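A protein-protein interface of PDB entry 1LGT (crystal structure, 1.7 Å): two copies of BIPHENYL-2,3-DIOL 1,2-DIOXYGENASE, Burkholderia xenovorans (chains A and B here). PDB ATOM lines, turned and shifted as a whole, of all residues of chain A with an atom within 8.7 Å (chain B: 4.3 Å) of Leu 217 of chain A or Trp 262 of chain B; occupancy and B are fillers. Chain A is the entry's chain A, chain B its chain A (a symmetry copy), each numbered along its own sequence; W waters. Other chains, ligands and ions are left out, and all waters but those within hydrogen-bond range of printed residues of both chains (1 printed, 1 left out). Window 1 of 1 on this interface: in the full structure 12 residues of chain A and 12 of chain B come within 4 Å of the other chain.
Water W1 bridges NH2 of Arg 239 of chain A (3.2 Å) and N of Leu 217 of chain B (3.4 Å).
Gly 135 of chain A touches none of the printed residues of chain B. Leu 217 of chain A touches just these residues of chain B: Arg 239 (3.96 Å) and Trp 262 (3.9 Å). Printed residues of chain B within 4 Å of Asp 218 of chain A: Arg 239 and Trp 282. Met 245 of chain A touches none of the printed residues of chain B. Printed residues of chain B within 4 Å of Trp 262 of chain A: Leu 217. Printed residues of chain A within 4 Å of Arg 239 of chain B: Leu 217 (3.96 Å) and Asp 218 (2.6 Å). No residue of chain A comes within 4 Å of Val 246 of chain B. No residue of chain A comes within 4 Å of Gly 261 of chain B. Of the printed residues of chain A, Trp 262 of chain B touches Leu 217 (3.9 Å). No residue of chain A comes within 4 Å of Ser 263 of chain B. The nearest residue of chain B that does not touch Leu 217 of chain A is Val 246 of chain B (4.04 Å).
Among the printed residues, merely in contact across the chains: Leu 217 of chain A with Arg 239 of chain B (3.96 Å), Leu 217 of chain A with Trp 262 of chain B (3.9 Å), Gly 221 of chain A with Trp 282 of chain B (3.5 Å), Phe 222 of chain A with Trp 282 of chain B (3.96 Å), Arg 239 of chain A with Leu 217 of chain B (3.96 Å) and Trp 262 of chain A with Leu 217 of chain B (3.9 Å).
Of the 13 printed residues of chain B, 4 touch a printed residue of chain A. Hydrophobic or aromatic side chains of chain B that line the printed part of chain A: Leu 217, Trp 262 and Trp 282. Of the 25 printed residues of chain A, 6 touch a printed residue of chain B. Among the printed residues, 8 pairs touch across the chains.
OD1 of Asp 218 of chain A lies within salt-bridge range of NE of Arg 239 of chain B (2.6 Å). The side-chain carboxylate of Asp 218 of chain A is in hydrogen-bond range of the indole nitrogen of Trp 282 of chain B (2.8 Å).
The backbone carbonyl oxygen (O) of Ala 215 of chain A sits at hydrogen-bond distance from the indole nitrogen (NE1) of Trp 262 of chain A. The backbone NH (N) of Arg 239 of chain A lies within hydrogen-bond range of the backbone carbonyl oxygen (O) of Trp 282 of chain A. N of Trp 262 of chain A lies within hydrogen-bond range of O of Val 246 of chain A. The backbone carbonyl oxygen (O) of Ala 215 of chain B sits at hydrogen-bond distance from the indole nitrogen (NE1) of Trp 262 of chain B, at 3.4 Å. N of Arg 239 of chain B sits at hydrogen-bond distance from O of Trp 282 of chain B (3.0 Å). The backbone carbonyl oxygen (O) of Val 246 of chain B is in hydrogen-bond range of the backbone NH (N) of Trp 262 of chain B.
Leu 217 of chain A touches Arg 239 of chain B, and with the chains exchanged Arg 239 of chain A touches Leu 217 of chain B. Leu 217 of chain A touches Trp 262 of chain B, and with the chains exchanged Trp 262 of chain A touches Leu 217 of chain B. Of the 8 pairs that touch across the chains among the printed residues, 4 have their exchanged pair printed and touching as well.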
ATOM      1  N   SER A 134     -32.069  -1.376   3.979  1.00  0.00           N
ATOM      2  CA  SER A 134     -32.140  -2.198   2.771  1.00  0.00           C
ATOM      3  C   SER A 134     -31.455  -3.547   2.945  1.00  0.00           C
ATOM      4  O   SER A 134     -31.781  -4.511   2.248  1.00  0.00           O
ATOM      5  CB  SER A 134     -31.539  -1.452   1.571  1.00  0.00           C
ATOM      6  OG  SER A 134     -30.128  -1.390   1.640  1.00  0.00           O
ATOM      7  N   GLY A 135     -30.511  -3.619   3.879  1.00  0.00           N
ATOM      8  CA  GLY A 135     -29.818  -4.872   4.123  1.00  0.00           C
ATOM      9  C   GLY A 135     -28.471  -4.690   4.792  1.00  0.00           C
ATOM     10  O   GLY A 135     -27.892  -3.599   4.763  1.00  0.00           O
ATOM     11  N   VAL A 214     -23.901  -1.824   6.244  1.00  0.00           N
ATOM     12  CA  VAL A 214     -25.169  -1.886   5.528  1.00  0.00           C
ATOM     13  C   VAL A 214     -24.980  -1.759   4.020  1.00  0.00           C
ATOM     14  O   VAL A 214     -23.896  -1.409   3.548  1.00  0.00           O
ATOM     15  CB  VAL A 214     -26.157  -0.819   6.050  1.00  0.00           C
ATOM     16  CG1 VAL A 214     -26.641  -1.221   7.441  1.00  0.00           C
ATOM     17  CG2 VAL A 214     -25.481   0.547   6.106  1.00  0.00           C
ATOM     18  N   ALA A 215     -26.044  -2.034   3.273  1.00  0.00           N
ATOM     19  CA  ALA A 215     -25.990  -2.045   1.813  1.00  0.00           C
ATOM     20  C   ALA A 215     -26.083  -0.738   1.036  1.00  0.00           C
ATOM     21  O   ALA A 215     -25.680  -0.692  -0.126  1.00  0.00           O
ATOM     22  CB  ALA A 215     -27.044  -3.024   1.285  1.00  0.00           C
ATOM     23  N   SER A 216     -26.606   0.317   1.650  1.00  0.00           N
ATOM     24  CA  SER A 216     -26.745   1.586   0.943  1.00  0.00           C
ATOM     25  C   SER A 216     -26.314   2.778   1.781  1.00  0.00           C
ATOM     26  O   SER A 216     -26.284   2.705   3.012  1.00  0.00           O
ATOM     27  CB  SER A 216     -28.207   1.791   0.534  1.00  0.00           C
ATOM     28  OG  SER A 216     -28.703   0.663  -0.167  1.00  0.00           O
ATOM     29  N   LEU A 217     -25.985   3.878   1.109  1.00  0.00           N
ATOM     30  CA  LEU A 217     -25.607   5.094   1.817  1.00  0.00           C
ATOM     31  C   LEU A 217     -26.827   5.579   2.600  1.00  0.00           C
ATOM     32  O   LEU A 217     -26.694   6.067   3.723  1.00  0.00           O
ATOM     33  CB  LEU A 217     -25.168   6.181   0.834  1.00  0.00           C
ATOM     34  CG  LEU A 217     -24.971   7.583   1.424  1.00  0.00           C
ATOM     35  CD1 LEU A 217     -23.871   7.567   2.477  1.00  0.00           C
ATOM     36  CD2 LEU A 217     -24.616   8.545   0.303  1.00  0.00           C
ATOM     37  N   ASP A 218     -28.014   5.450   2.008  1.00  0.00           N
ATOM     38  CA  ASP A 218     -29.232   5.873   2.694  1.00  0.00           C
ATOM     39  C   ASP A 218     -29.448   5.108   4.000  1.00  0.00           C
ATOM     40  O   ASP A 218     -29.967   5.669   4.966  1.00  0.00           O
ATOM     41  CB  ASP A 218     -30.461   5.706   1.796  1.00  0.00           C
ATOM     42  CG  ASP A 218     -30.536   6.760   0.714  1.00  0.00           C
ATOM     43  OD1 ASP A 218     -30.002   7.869   0.933  1.00  0.00           O
ATOM     44  OD2 ASP A 218     -31.143   6.487  -0.345  1.00  0.00           O
ATOM     45  N   ASP A 219     -29.066   3.834   4.037  1.00  0.00           N
ATOM     46  CA  ASP A 219     -29.230   3.067   5.273  1.00  0.00           C
ATOM     47  C   ASP A 219     -28.464   3.778   6.387  1.00  0.00           C
ATOM     48  O   ASP A 219     -28.956   3.905   7.509  1.00  0.00           O
ATOM     49  CB  ASP A 219     -28.693   1.641   5.127  1.00  0.00           C
ATOM     50  CG  ASP A 219     -29.510   0.803   4.161  1.00  0.00           C
ATOM     51  OD1 ASP A 219     -30.725   1.063   4.037  1.00  0.00           O
ATOM     52  OD2 ASP A 219     -28.940  -0.128   3.546  1.00  0.00           O
ATOM     53  N   VAL A 220     -27.259   4.238   6.063  1.00  0.00           N
ATOM     54  CA  VAL A 220     -26.423   4.950   7.024  1.00  0.00           C
ATOM     55  C   VAL A 220     -27.012   6.326   7.348  1.00  0.00           C
ATOM     56  O   VAL A 220     -27.098   6.713   8.515  1.00  0.00           O
ATOM     57  CB  VAL A 220     -24.982   5.127   6.476  1.00  0.00           C
ATOM     58  CG1 VAL A 220     -24.127   5.875   7.481  1.00  0.00           C
ATOM     59  CG2 VAL A 220     -24.364   3.761   6.183  1.00  0.00           C
ATOM     60  N   GLY A 221     -27.423   7.056   6.315  1.00  0.00           N
ATOM     61  CA  GLY A 221     -27.990   8.384   6.509  1.00  0.00           C
ATOM     62  C   GLY A 221     -29.224   8.412   7.395  1.00  0.00           C
ATOM     63  O   GLY A 221     -29.351   9.267   8.284  1.00  0.00           O
ATOM     64  N   PHE A 222     -30.144   7.487   7.152  1.00  0.00           N
ATOM     65  CA  PHE A 222     -31.367   7.411   7.944  1.00  0.00           C
ATOM     66  C   PHE A 222     -31.051   7.007   9.383  1.00  0.00           C
ATOM     67  O   PHE A 222     -31.613   7.568  10.327  1.00  0.00           O
ATOM     68  CB  PHE A 222     -32.344   6.401   7.328  1.00  0.00           C
ATOM     69  CG  PHE A 222     -33.088   6.920   6.127  1.00  0.00           C
ATOM     70  CD1 PHE A 222     -33.894   8.053   6.226  1.00  0.00           C
ATOM     71  CD2 PHE A 222     -33.013   6.257   4.904  1.00  0.00           C
ATOM     72  CE1 PHE A 222     -34.620   8.517   5.123  1.00  0.00           C
ATOM     73  CE2 PHE A 222     -33.735   6.713   3.796  1.00  0.00           C
ATOM     74  CZ  PHE A 222     -34.539   7.843   3.908  1.00  0.00           C
ATOM     75  N   ALA A 223     -30.154   6.036   9.550  1.00  0.00           N
ATOM     76  CA  ALA A 223     -29.781   5.570  10.880  1.00  0.00           C
ATOM     77  C   ALA A 223     -29.149   6.703  11.676  1.00  0.00           C
ATOM     78  O   ALA A 223     -29.406   6.855  12.871  1.00  0.00           O
ATOM     79  CB  ALA A 223     -28.811   4.401  10.782  1.00  0.00           C
ATOM     80  N   PHE A 224     -28.320   7.501  11.010  1.00  0.00           N
ATOM     81  CA  PHE A 224     -27.669   8.625  11.673  1.00  0.00           C
ATOM     82  C   PHE A 224     -28.730   9.517  12.317  1.00  0.00           C
ATOM     83  O   PHE A 224     -28.627   9.878  13.493  1.00  0.00           O
ATOM     84  CB  PHE A 224     -26.843   9.422  10.654  1.00  0.00           C
ATOM     85  CG  PHE A 224     -26.042  10.544  11.258  1.00  0.00           C
ATOM     86  CD1 PHE A 224     -26.656  11.734  11.637  1.00  0.00           C
ATOM     87  CD2 PHE A 224     -24.670  10.410  11.445  1.00  0.00           C
ATOM     88  CE1 PHE A 224     -25.913  12.778  12.193  1.00  0.00           C
ATOM     89  CE2 PHE A 224     -23.916  11.450  12.003  1.00  0.00           C
ATOM     90  CZ  PHE A 224     -24.547  12.636  12.376  1.00  0.00           C
ATOM     91  N   LEU A 237     -20.617  11.865  10.041  1.00  0.00           N
ATOM     92  CA  LEU A 237     -20.348  11.002   8.895  1.00  0.00           C
ATOM     93  C   LEU A 237     -18.953  11.285   8.346  1.00  0.00           C
ATOM     94  O   LEU A 237     -18.541  12.441   8.235  1.00  0.00           O
ATOM     95  CB  LEU A 237     -21.383  11.240   7.795  1.00  0.00           C
ATOM     96  CG  LEU A 237     -22.815  10.773   8.050  1.00  0.00           C
ATOM     97  CD1 LEU A 237     -23.716  11.271   6.933  1.00  0.00           C
ATOM     98  CD2 LEU A 237     -22.849   9.250   8.123  1.00  0.00           C
ATOM     99  N   GLY A 238     -18.232  10.223   8.013  1.00  0.00           N
ATOM    100  CA  GLY A 238     -16.895  10.374   7.466  1.00  0.00           C
ATOM    101  C   GLY A 238     -16.489   9.109   6.734  1.00  0.00           C
ATOM    102  O   GLY A 238     -17.232   8.125   6.735  1.00  0.00           O
ATOM    103  N   ARG A 239     -15.323   9.135   6.096  1.00  0.00           N
ATOM    104  CA  ARG A 239     -14.822   7.961   5.391  1.00  0.00           C
ATOM    105  C   ARG A 239     -13.427   7.667   5.908  1.00  0.00           C
ATOM    106  O   ARG A 239     -12.592   8.567   6.003  1.00  0.00           O
ATOM    107  CB  ARG A 239     -14.755   8.178   3.871  1.00  0.00           C
ATOM    108  CG  ARG A 239     -14.458   6.861   3.134  1.00  0.00           C
ATOM    109  CD  ARG A 239     -13.977   7.040   1.695  1.00  0.00           C
ATOM    110  NE  ARG A 239     -15.005   7.459   0.745  1.00  0.00           N
ATOM    111  CZ  ARG A 239     -15.861   6.642   0.134  1.00  0.00           C
ATOM    112  NH1 ARG A 239     -15.840   5.338   0.371  1.00  0.00           N
ATOM    113  NH2 ARG A 239     -16.721   7.131  -0.748  1.00  0.00           N
ATOM    114  N   MET A 245     -14.404   2.981   4.414  1.00  0.00           N
ATOM    115  CA  MET A 245     -15.803   2.849   4.778  1.00  0.00           C
ATOM    116  C   MET A 245     -16.372   4.211   5.155  1.00  0.00           C
ATOM    117  O   MET A 245     -15.695   5.010   5.810  1.00  0.00           O
ATOM    118  CB  MET A 245     -15.956   1.904   5.971  1.00  0.00           C
ATOM    119  CG  MET A 245     -17.389   1.797   6.458  1.00  0.00           C
ATOM    120  SD  MET A 245     -17.553   0.642   7.812  1.00  0.00           S
ATOM    121  CE  MET A 245     -17.257  -0.926   6.944  1.00  0.00           C
ATOM    122  N   VAL A 246     -17.604   4.472   4.728  1.00  0.00           N
ATOM    123  CA  VAL A 246     -18.298   5.714   5.066  1.00  0.00           C
ATOM    124  C   VAL A 246     -19.155   5.314   6.261  1.00  0.00           C
ATOM    125  O   VAL A 246     -19.984   4.410   6.154  1.00  0.00           O
ATOM    126  CB  VAL A 246     -19.210   6.192   3.918  1.00  0.00           C
ATOM    127  CG1 VAL A 246     -20.022   7.398   4.368  1.00  0.00           C
ATOM    128  CG2 VAL A 246     -18.360   6.565   2.703  1.00  0.00           C
ATOM    129  N   SER A 247     -18.970   5.983   7.395  1.00  0.00           N
ATOM    130  CA  SER A 247     -19.713   5.605   8.590  1.00  0.00           C
ATOM    131  C   SER A 247     -19.841   6.728   9.601  1.00  0.00           C
ATOM    132  O   SER A 247     -19.329   7.826   9.404  1.00  0.00           O
ATOM    133  CB  SER A 247     -18.979   4.463   9.285  1.00  0.00           C
ATOM    134  OG  SER A 247     -17.715   4.923   9.765  1.00  0.00           O
ATOM    135  N   PHE A 248     -20.548   6.426  10.685  1.00  0.00           N
ATOM    136  CA  PHE A 248     -20.677   7.346  11.808  1.00  0.00           C
ATOM    137  C   PHE A 248     -20.582   6.459  13.041  1.00  0.00           C
ATOM    138  O   PHE A 248     -20.683   5.233  12.936  1.00  0.00           O
ATOM    139  CB  PHE A 248     -22.008   8.113  11.791  1.00  0.00           C
ATOM    140  CG  PHE A 248     -23.221   7.269  12.079  1.00  0.00           C
ATOM    141  CD1 PHE A 248     -23.627   7.022  13.390  1.00  0.00           C
ATOM    142  CD2 PHE A 248     -23.986   6.762  11.034  1.00  0.00           C
ATOM    143  CE1 PHE A 248     -24.788   6.285  13.654  1.00  0.00           C
ATOM    144  CE2 PHE A 248     -25.149   6.025  11.284  1.00  0.00           C
ATOM    145  CZ  PHE A 248     -25.550   5.788  12.599  1.00  0.00           C
ATOM    146  N   TYR A 260     -21.501   2.343  12.218  1.00  0.00           N
ATOM    147  CA  TYR A 260     -22.503   1.921  11.241  1.00  0.00           C
ATOM    148  C   TYR A 260     -22.018   2.466   9.901  1.00  0.00           C
ATOM    149  O   TYR A 260     -22.017   3.684   9.684  1.00  0.00           O
ATOM    150  CB  TYR A 260     -23.837   2.554  11.640  1.00  0.00           C
ATOM    151  CG  TYR A 260     -25.093   1.886  11.135  1.00  0.00           C
ATOM    152  CD1 TYR A 260     -25.619   0.759  11.775  1.00  0.00           C
ATOM    153  CD2 TYR A 260     -25.808   2.438  10.076  1.00  0.00           C
ATOM    154  CE1 TYR A 260     -26.848   0.212  11.373  1.00  0.00           C
ATOM    155  CE2 TYR A 260     -27.022   1.902   9.668  1.00  0.00           C
ATOM    156  CZ  TYR A 260     -27.539   0.800  10.320  1.00  0.00           C
ATOM    157  OH  TYR A 260     -28.773   0.326   9.929  1.00  0.00           O
ATOM    158  N   GLY A 261     -21.614   1.574   8.998  1.00  0.00           N
ATOM    159  CA  GLY A 261     -21.073   2.049   7.739  1.00  0.00           C
ATOM    160  C   GLY A 261     -21.464   1.379   6.443  1.00  0.00           C
ATOM    161  O   GLY A 261     -22.182   0.374   6.416  1.00  0.00           O
ATOM    162  N   TRP A 262     -20.931   1.941   5.361  1.00  0.00           N
ATOM    163  CA  TRP A 262     -21.227   1.484   4.011  1.00  0.00           C
ATOM    164  C   TRP A 262     -20.077   1.721   3.026  1.00  0.00           C
ATOM    165  O   TRP A 262     -19.298   2.659   3.181  1.00  0.00           O
ATOM    166  CB  TRP A 262     -22.475   2.237   3.525  1.00  0.00           C
ATOM    167  CG  TRP A 262     -22.685   2.259   2.032  1.00  0.00           C
ATOM    168  CD1 TRP A 262     -23.243   1.274   1.265  1.00  0.00           C
ATOM    169  CD2 TRP A 262     -22.348   3.326   1.134  1.00  0.00           C
ATOM    170  NE1 TRP A 262     -23.276   1.662  -0.053  1.00  0.00           N
ATOM    171  CE2 TRP A 262     -22.732   2.915  -0.164  1.00  0.00           C
ATOM    172  CE3 TRP A 262     -21.757   4.587   1.297  1.00  0.00           C
ATOM    173  CZ2 TRP A 262     -22.544   3.722  -1.295  1.00  0.00           C
ATOM    174  CZ3 TRP A 262     -21.570   5.392   0.169  1.00  0.00           C
ATOM    175  CH2 TRP A 262     -21.964   4.952  -1.108  1.00  0.00           C
ATOM    176  N   SER A 263     -19.982   0.839   2.030  1.00  0.00           N
ATOM    177  CA  SER A 263     -19.015   0.946   0.933  1.00  0.00           C
ATOM    178  C   SER A 263     -17.515   0.758   1.172  1.00  0.00           C
ATOM    179  O   SER A 263     -16.698   1.335   0.448  1.00  0.00           O
ATOM    180  CB  SER A 263     -19.244   2.283   0.217  1.00  0.00           C
ATOM    181  OG  SER A 263     -18.566   2.335  -1.028  1.00  0.00           O
ATOM    182  N   TRP A 282     -12.044  12.189   5.475  1.00  0.00           N
ATOM    183  CA  TRP A 282     -12.888  13.353   5.705  1.00  0.00           C
ATOM    184  C   TRP A 282     -13.962  13.001   6.719  1.00  0.00           C
ATOM    185  O   TRP A 282     -14.259  11.823   6.940  1.00  0.00           O
ATOM    186  CB  TRP A 282     -13.537  13.875   4.407  1.00  0.00           C
ATOM    187  CG  TRP A 282     -14.253  12.859   3.551  1.00  0.00           C
ATOM    188  CD1 TRP A 282     -13.745  12.206   2.462  1.00  0.00           C
ATOM    189  CD2 TRP A 282     -15.613  12.412   3.687  1.00  0.00           C
ATOM    190  NE1 TRP A 282     -14.699  11.387   1.912  1.00  0.00           N
ATOM    191  CE2 TRP A 282     -15.854  11.490   2.642  1.00  0.00           C
ATOM    192  CE3 TRP A 282     -16.647  12.699   4.589  1.00  0.00           C
ATOM    193  CZ2 TRP A 282     -17.089  10.853   2.471  1.00  0.00           C
ATOM    194  CZ3 TRP A 282     -17.883  12.063   4.419  1.00  0.00           C
ATOM    195  CH2 TRP A 282     -18.088  11.150   3.365  1.00  0.00           C
ATOM    196  N   VAL B 214     -20.834  17.693  -8.191  1.00  0.00           N
ATOM    197  CA  VAL B 214     -19.559  17.034  -8.447  1.00  0.00           C
ATOM    198  C   VAL B 214     -19.735  15.553  -8.766  1.00  0.00           C
ATOM    199  O   VAL B 214     -20.817  14.992  -8.580  1.00  0.00           O
ATOM    200  CB  VAL B 214     -18.584  17.230  -7.265  1.00  0.00           C
ATOM    201  CG1 VAL B 214     -18.110  18.681  -7.239  1.00  0.00           C
ATOM    202  CG2 VAL B 214     -19.270  16.880  -5.948  1.00  0.00           C
ATOM    203  N   ALA B 215     -18.661  14.926  -9.237  1.00  0.00           N
ATOM    204  CA  ALA B 215     -18.702  13.533  -9.673  1.00  0.00           C
ATOM    205  C   ALA B 215     -18.611  12.409  -8.649  1.00  0.00           C
ATOM    206  O   ALA B 215     -19.003  11.281  -8.947  1.00  0.00           O
ATOM    207  CB  ALA B 215     -17.636  13.320 -10.754  1.00  0.00           C
ATOM    208  N   SER B 216     -18.101  12.692  -7.455  1.00  0.00           N
ATOM    209  CA  SER B 216     -17.964  11.647  -6.446  1.00  0.00           C
ATOM    210  C   SER B 216     -18.411  12.099  -5.066  1.00  0.00           C
ATOM    211  O   SER B 216     -18.452  13.298  -4.777  1.00  0.00           O
ATOM    212  CB  SER B 216     -16.500  11.207  -6.355  1.00  0.00           C
ATOM    213  OG  SER B 216     -15.989  10.868  -7.634  1.00  0.00           O
ATOM    214  N   LEU B 217     -18.742  11.133  -4.213  1.00  0.00           N
ATOM    215  CA  LEU B 217     -19.135  11.453  -2.846  1.00  0.00           C
ATOM    216  C   LEU B 217     -17.926  12.070  -2.143  1.00  0.00           C
ATOM    217  O   LEU B 217     -18.073  13.001  -1.351  1.00  0.00           O
ATOM    218  CB  LEU B 217     -19.573  10.193  -2.097  1.00  0.00           C
ATOM    219  CG  LEU B 217     -19.785  10.348  -0.586  1.00  0.00           C
ATOM    220  CD1 LEU B 217     -20.895  11.352  -0.306  1.00  0.00           C
ATOM    221  CD2 LEU B 217     -20.136   8.993   0.004  1.00  0.00           C
ATOM    222  N   VAL B 220     -17.517  15.776  -2.413  1.00  0.00           N
ATOM    223  CA  VAL B 220     -18.368  16.482  -1.460  1.00  0.00           C
ATOM    224  C   VAL B 220     -17.791  16.395  -0.043  1.00  0.00           C
ATOM    225  O   VAL B 220     -17.718  17.400   0.667  1.00  0.00           O
ATOM    226  CB  VAL B 220     -19.804  15.897  -1.464  1.00  0.00           C
ATOM    227  CG1 VAL B 220     -20.673  16.634  -0.463  1.00  0.00           C
ATOM    228  CG2 VAL B 220     -20.410  16.010  -2.862  1.00  0.00           C
ATOM    229  N   ARG B 239     -29.487  14.297   2.168  1.00  0.00           N
ATOM    230  CA  ARG B 239     -29.973  13.961   0.835  1.00  0.00           C
ATOM    231  C   ARG B 239     -31.371  14.532   0.691  1.00  0.00           C
ATOM    232  O   ARG B 239     -32.213  14.354   1.572  1.00  0.00           O
ATOM    233  CB  ARG B 239     -30.028  12.444   0.599  1.00  0.00           C
ATOM    234  CG  ARG B 239     -30.308  12.120  -0.878  1.00  0.00           C
ATOM    235  CD  ARG B 239     -30.777  10.689  -1.131  1.00  0.00           C
ATOM    236  NE  ARG B 239     -29.743   9.665  -0.997  1.00  0.00           N
ATOM    237  CZ  ARG B 239     -28.875   9.325  -1.948  1.00  0.00           C
ATOM    238  NH1 ARG B 239     -28.889   9.931  -3.127  1.00  0.00           N
ATOM    239  NH2 ARG B 239     -28.010   8.344  -1.729  1.00  0.00           N
ATOM    240  N   MET B 245     -30.347  14.475  -4.218  1.00  0.00           N
ATOM    241  CA  MET B 245     -28.951  14.871  -4.224  1.00  0.00           C
ATOM    242  C   MET B 245     -28.395  14.839  -2.806  1.00  0.00           C
ATOM    243  O   MET B 245     -29.083  15.228  -1.858  1.00  0.00           O
ATOM    244  CB  MET B 245     -28.802  16.289  -4.779  1.00  0.00           C
ATOM    245  CG  MET B 245     -27.373  16.797  -4.726  1.00  0.00           C
ATOM    246  SD  MET B 245     -27.214  18.429  -5.435  1.00  0.00           S
ATOM    247  CE  MET B 245     -27.491  18.054  -7.191  1.00  0.00           C
ATOM    248  N   VAL B 246     -27.161  14.363  -2.669  1.00  0.00           N
ATOM    249  CA  VAL B 246     -26.479  14.330  -1.376  1.00  0.00           C
ATOM    250  C   VAL B 246     -25.630  15.596  -1.402  1.00  0.00           C
ATOM    251  O   VAL B 246     -24.794  15.762  -2.290  1.00  0.00           O
ATOM    252  CB  VAL B 246     -25.559  13.099  -1.245  1.00  0.00           C
ATOM    253  CG1 VAL B 246     -24.760  13.184   0.048  1.00  0.00           C
ATOM    254  CG2 VAL B 246     -26.400  11.822  -1.250  1.00  0.00           C
ATOM    255  N   GLY B 261     -23.171  19.321  -4.160  1.00  0.00           N
ATOM    256  CA  GLY B 261     -23.703  17.974  -4.077  1.00  0.00           C
ATOM    257  C   GLY B 261     -23.296  16.932  -5.092  1.00  0.00           C
ATOM    258  O   GLY B 261     -22.570  17.205  -6.054  1.00  0.00           O
ATOM    259  N   TRP B 262     -23.822  15.730  -4.875  1.00  0.00           N
ATOM    260  CA  TRP B 262     -23.510  14.573  -5.702  1.00  0.00           C
ATOM    261  C   TRP B 262     -24.652  13.554  -5.773  1.00  0.00           C
ATOM    262  O   TRP B 262     -25.439  13.423  -4.839  1.00  0.00           O
ATOM    263  CB  TRP B 262     -22.263  13.898  -5.111  1.00  0.00           C
ATOM    264  CG  TRP B 262     -22.039  12.465  -5.523  1.00  0.00           C
ATOM    265  CD1 TRP B 262     -21.467  12.022  -6.684  1.00  0.00           C
ATOM    266  CD2 TRP B 262     -22.375  11.293  -4.768  1.00  0.00           C
ATOM    267  NE1 TRP B 262     -21.424  10.648  -6.696  1.00  0.00           N
ATOM    268  CE2 TRP B 262     -21.976  10.174  -5.535  1.00  0.00           C
ATOM    269  CE3 TRP B 262     -22.977  11.077  -3.519  1.00  0.00           C
ATOM    270  CZ2 TRP B 262     -22.159   8.855  -5.095  1.00  0.00           C
ATOM    271  CZ3 TRP B 262     -23.158   9.762  -3.080  1.00  0.00           C
ATOM    272  CH2 TRP B 262     -22.749   8.671  -3.869  1.00  0.00           C
ATOM    273  N   SER B 263     -24.732  12.857  -6.908  1.00  0.00           N
ATOM    274  CA  SER B 263     -25.689  11.771  -7.135  1.00  0.00           C
ATOM    275  C   SER B 263     -27.190  12.043  -7.258  1.00  0.00           C
ATOM    276  O   SER B 263     -28.004  11.177  -6.926  1.00  0.00           O
ATOM    277  CB  SER B 263     -25.463  10.698  -6.062  1.00  0.00           C
ATOM    278  OG  SER B 263     -26.129   9.487  -6.381  1.00  0.00           O
ATOM    279  N   ALA B 264     -27.572  13.213  -7.754  1.00  0.00           N
ATOM    280  CA  ALA B 264     -28.992  13.512  -7.911  1.00  0.00           C
ATOM    281  C   ALA B 264     -29.599  12.676  -9.038  1.00  0.00           C
ATOM    282  O   ALA B 264     -28.896  12.264  -9.970  1.00  0.00           O
ATOM    283  CB  ALA B 264     -29.185  14.987  -8.211  1.00  0.00           C
ATOM    284  N   TRP B 282     -32.781  12.790   4.878  1.00  0.00           N
ATOM    285  CA  TRP B 282     -31.947  12.678   6.066  1.00  0.00           C
ATOM    286  C   TRP B 282     -30.881  13.757   6.035  1.00  0.00           C
ATOM    287  O   TRP B 282     -30.578  14.313   4.975  1.00  0.00           O
ATOM    288  CB  TRP B 282     -31.290  11.288   6.193  1.00  0.00           C
ATOM    289  CG  TRP B 282     -30.559  10.770   4.979  1.00  0.00           C
ATOM    290  CD1 TRP B 282     -31.052   9.915   4.032  1.00  0.00           C
ATOM    291  CD2 TRP B 282     -29.197  11.040   4.604  1.00  0.00           C
ATOM    292  NE1 TRP B 282     -30.087   9.635   3.098  1.00  0.00           N
ATOM    293  CE2 TRP B 282     -28.940  10.311   3.420  1.00  0.00           C
ATOM    294  CE3 TRP B 282     -28.173  11.826   5.151  1.00  0.00           C
ATOM    295  CZ2 TRP B 282     -27.699  10.341   2.772  1.00  0.00           C
ATOM    296  CZ3 TRP B 282     -26.932  11.858   4.504  1.00  0.00           C
ATOM    297  CH2 TRP B 282     -26.710  11.117   3.326  1.00  0.00           C
HETATM  298  O   HOH W   1     -16.355   8.816  -3.438  1.00  0.00           O
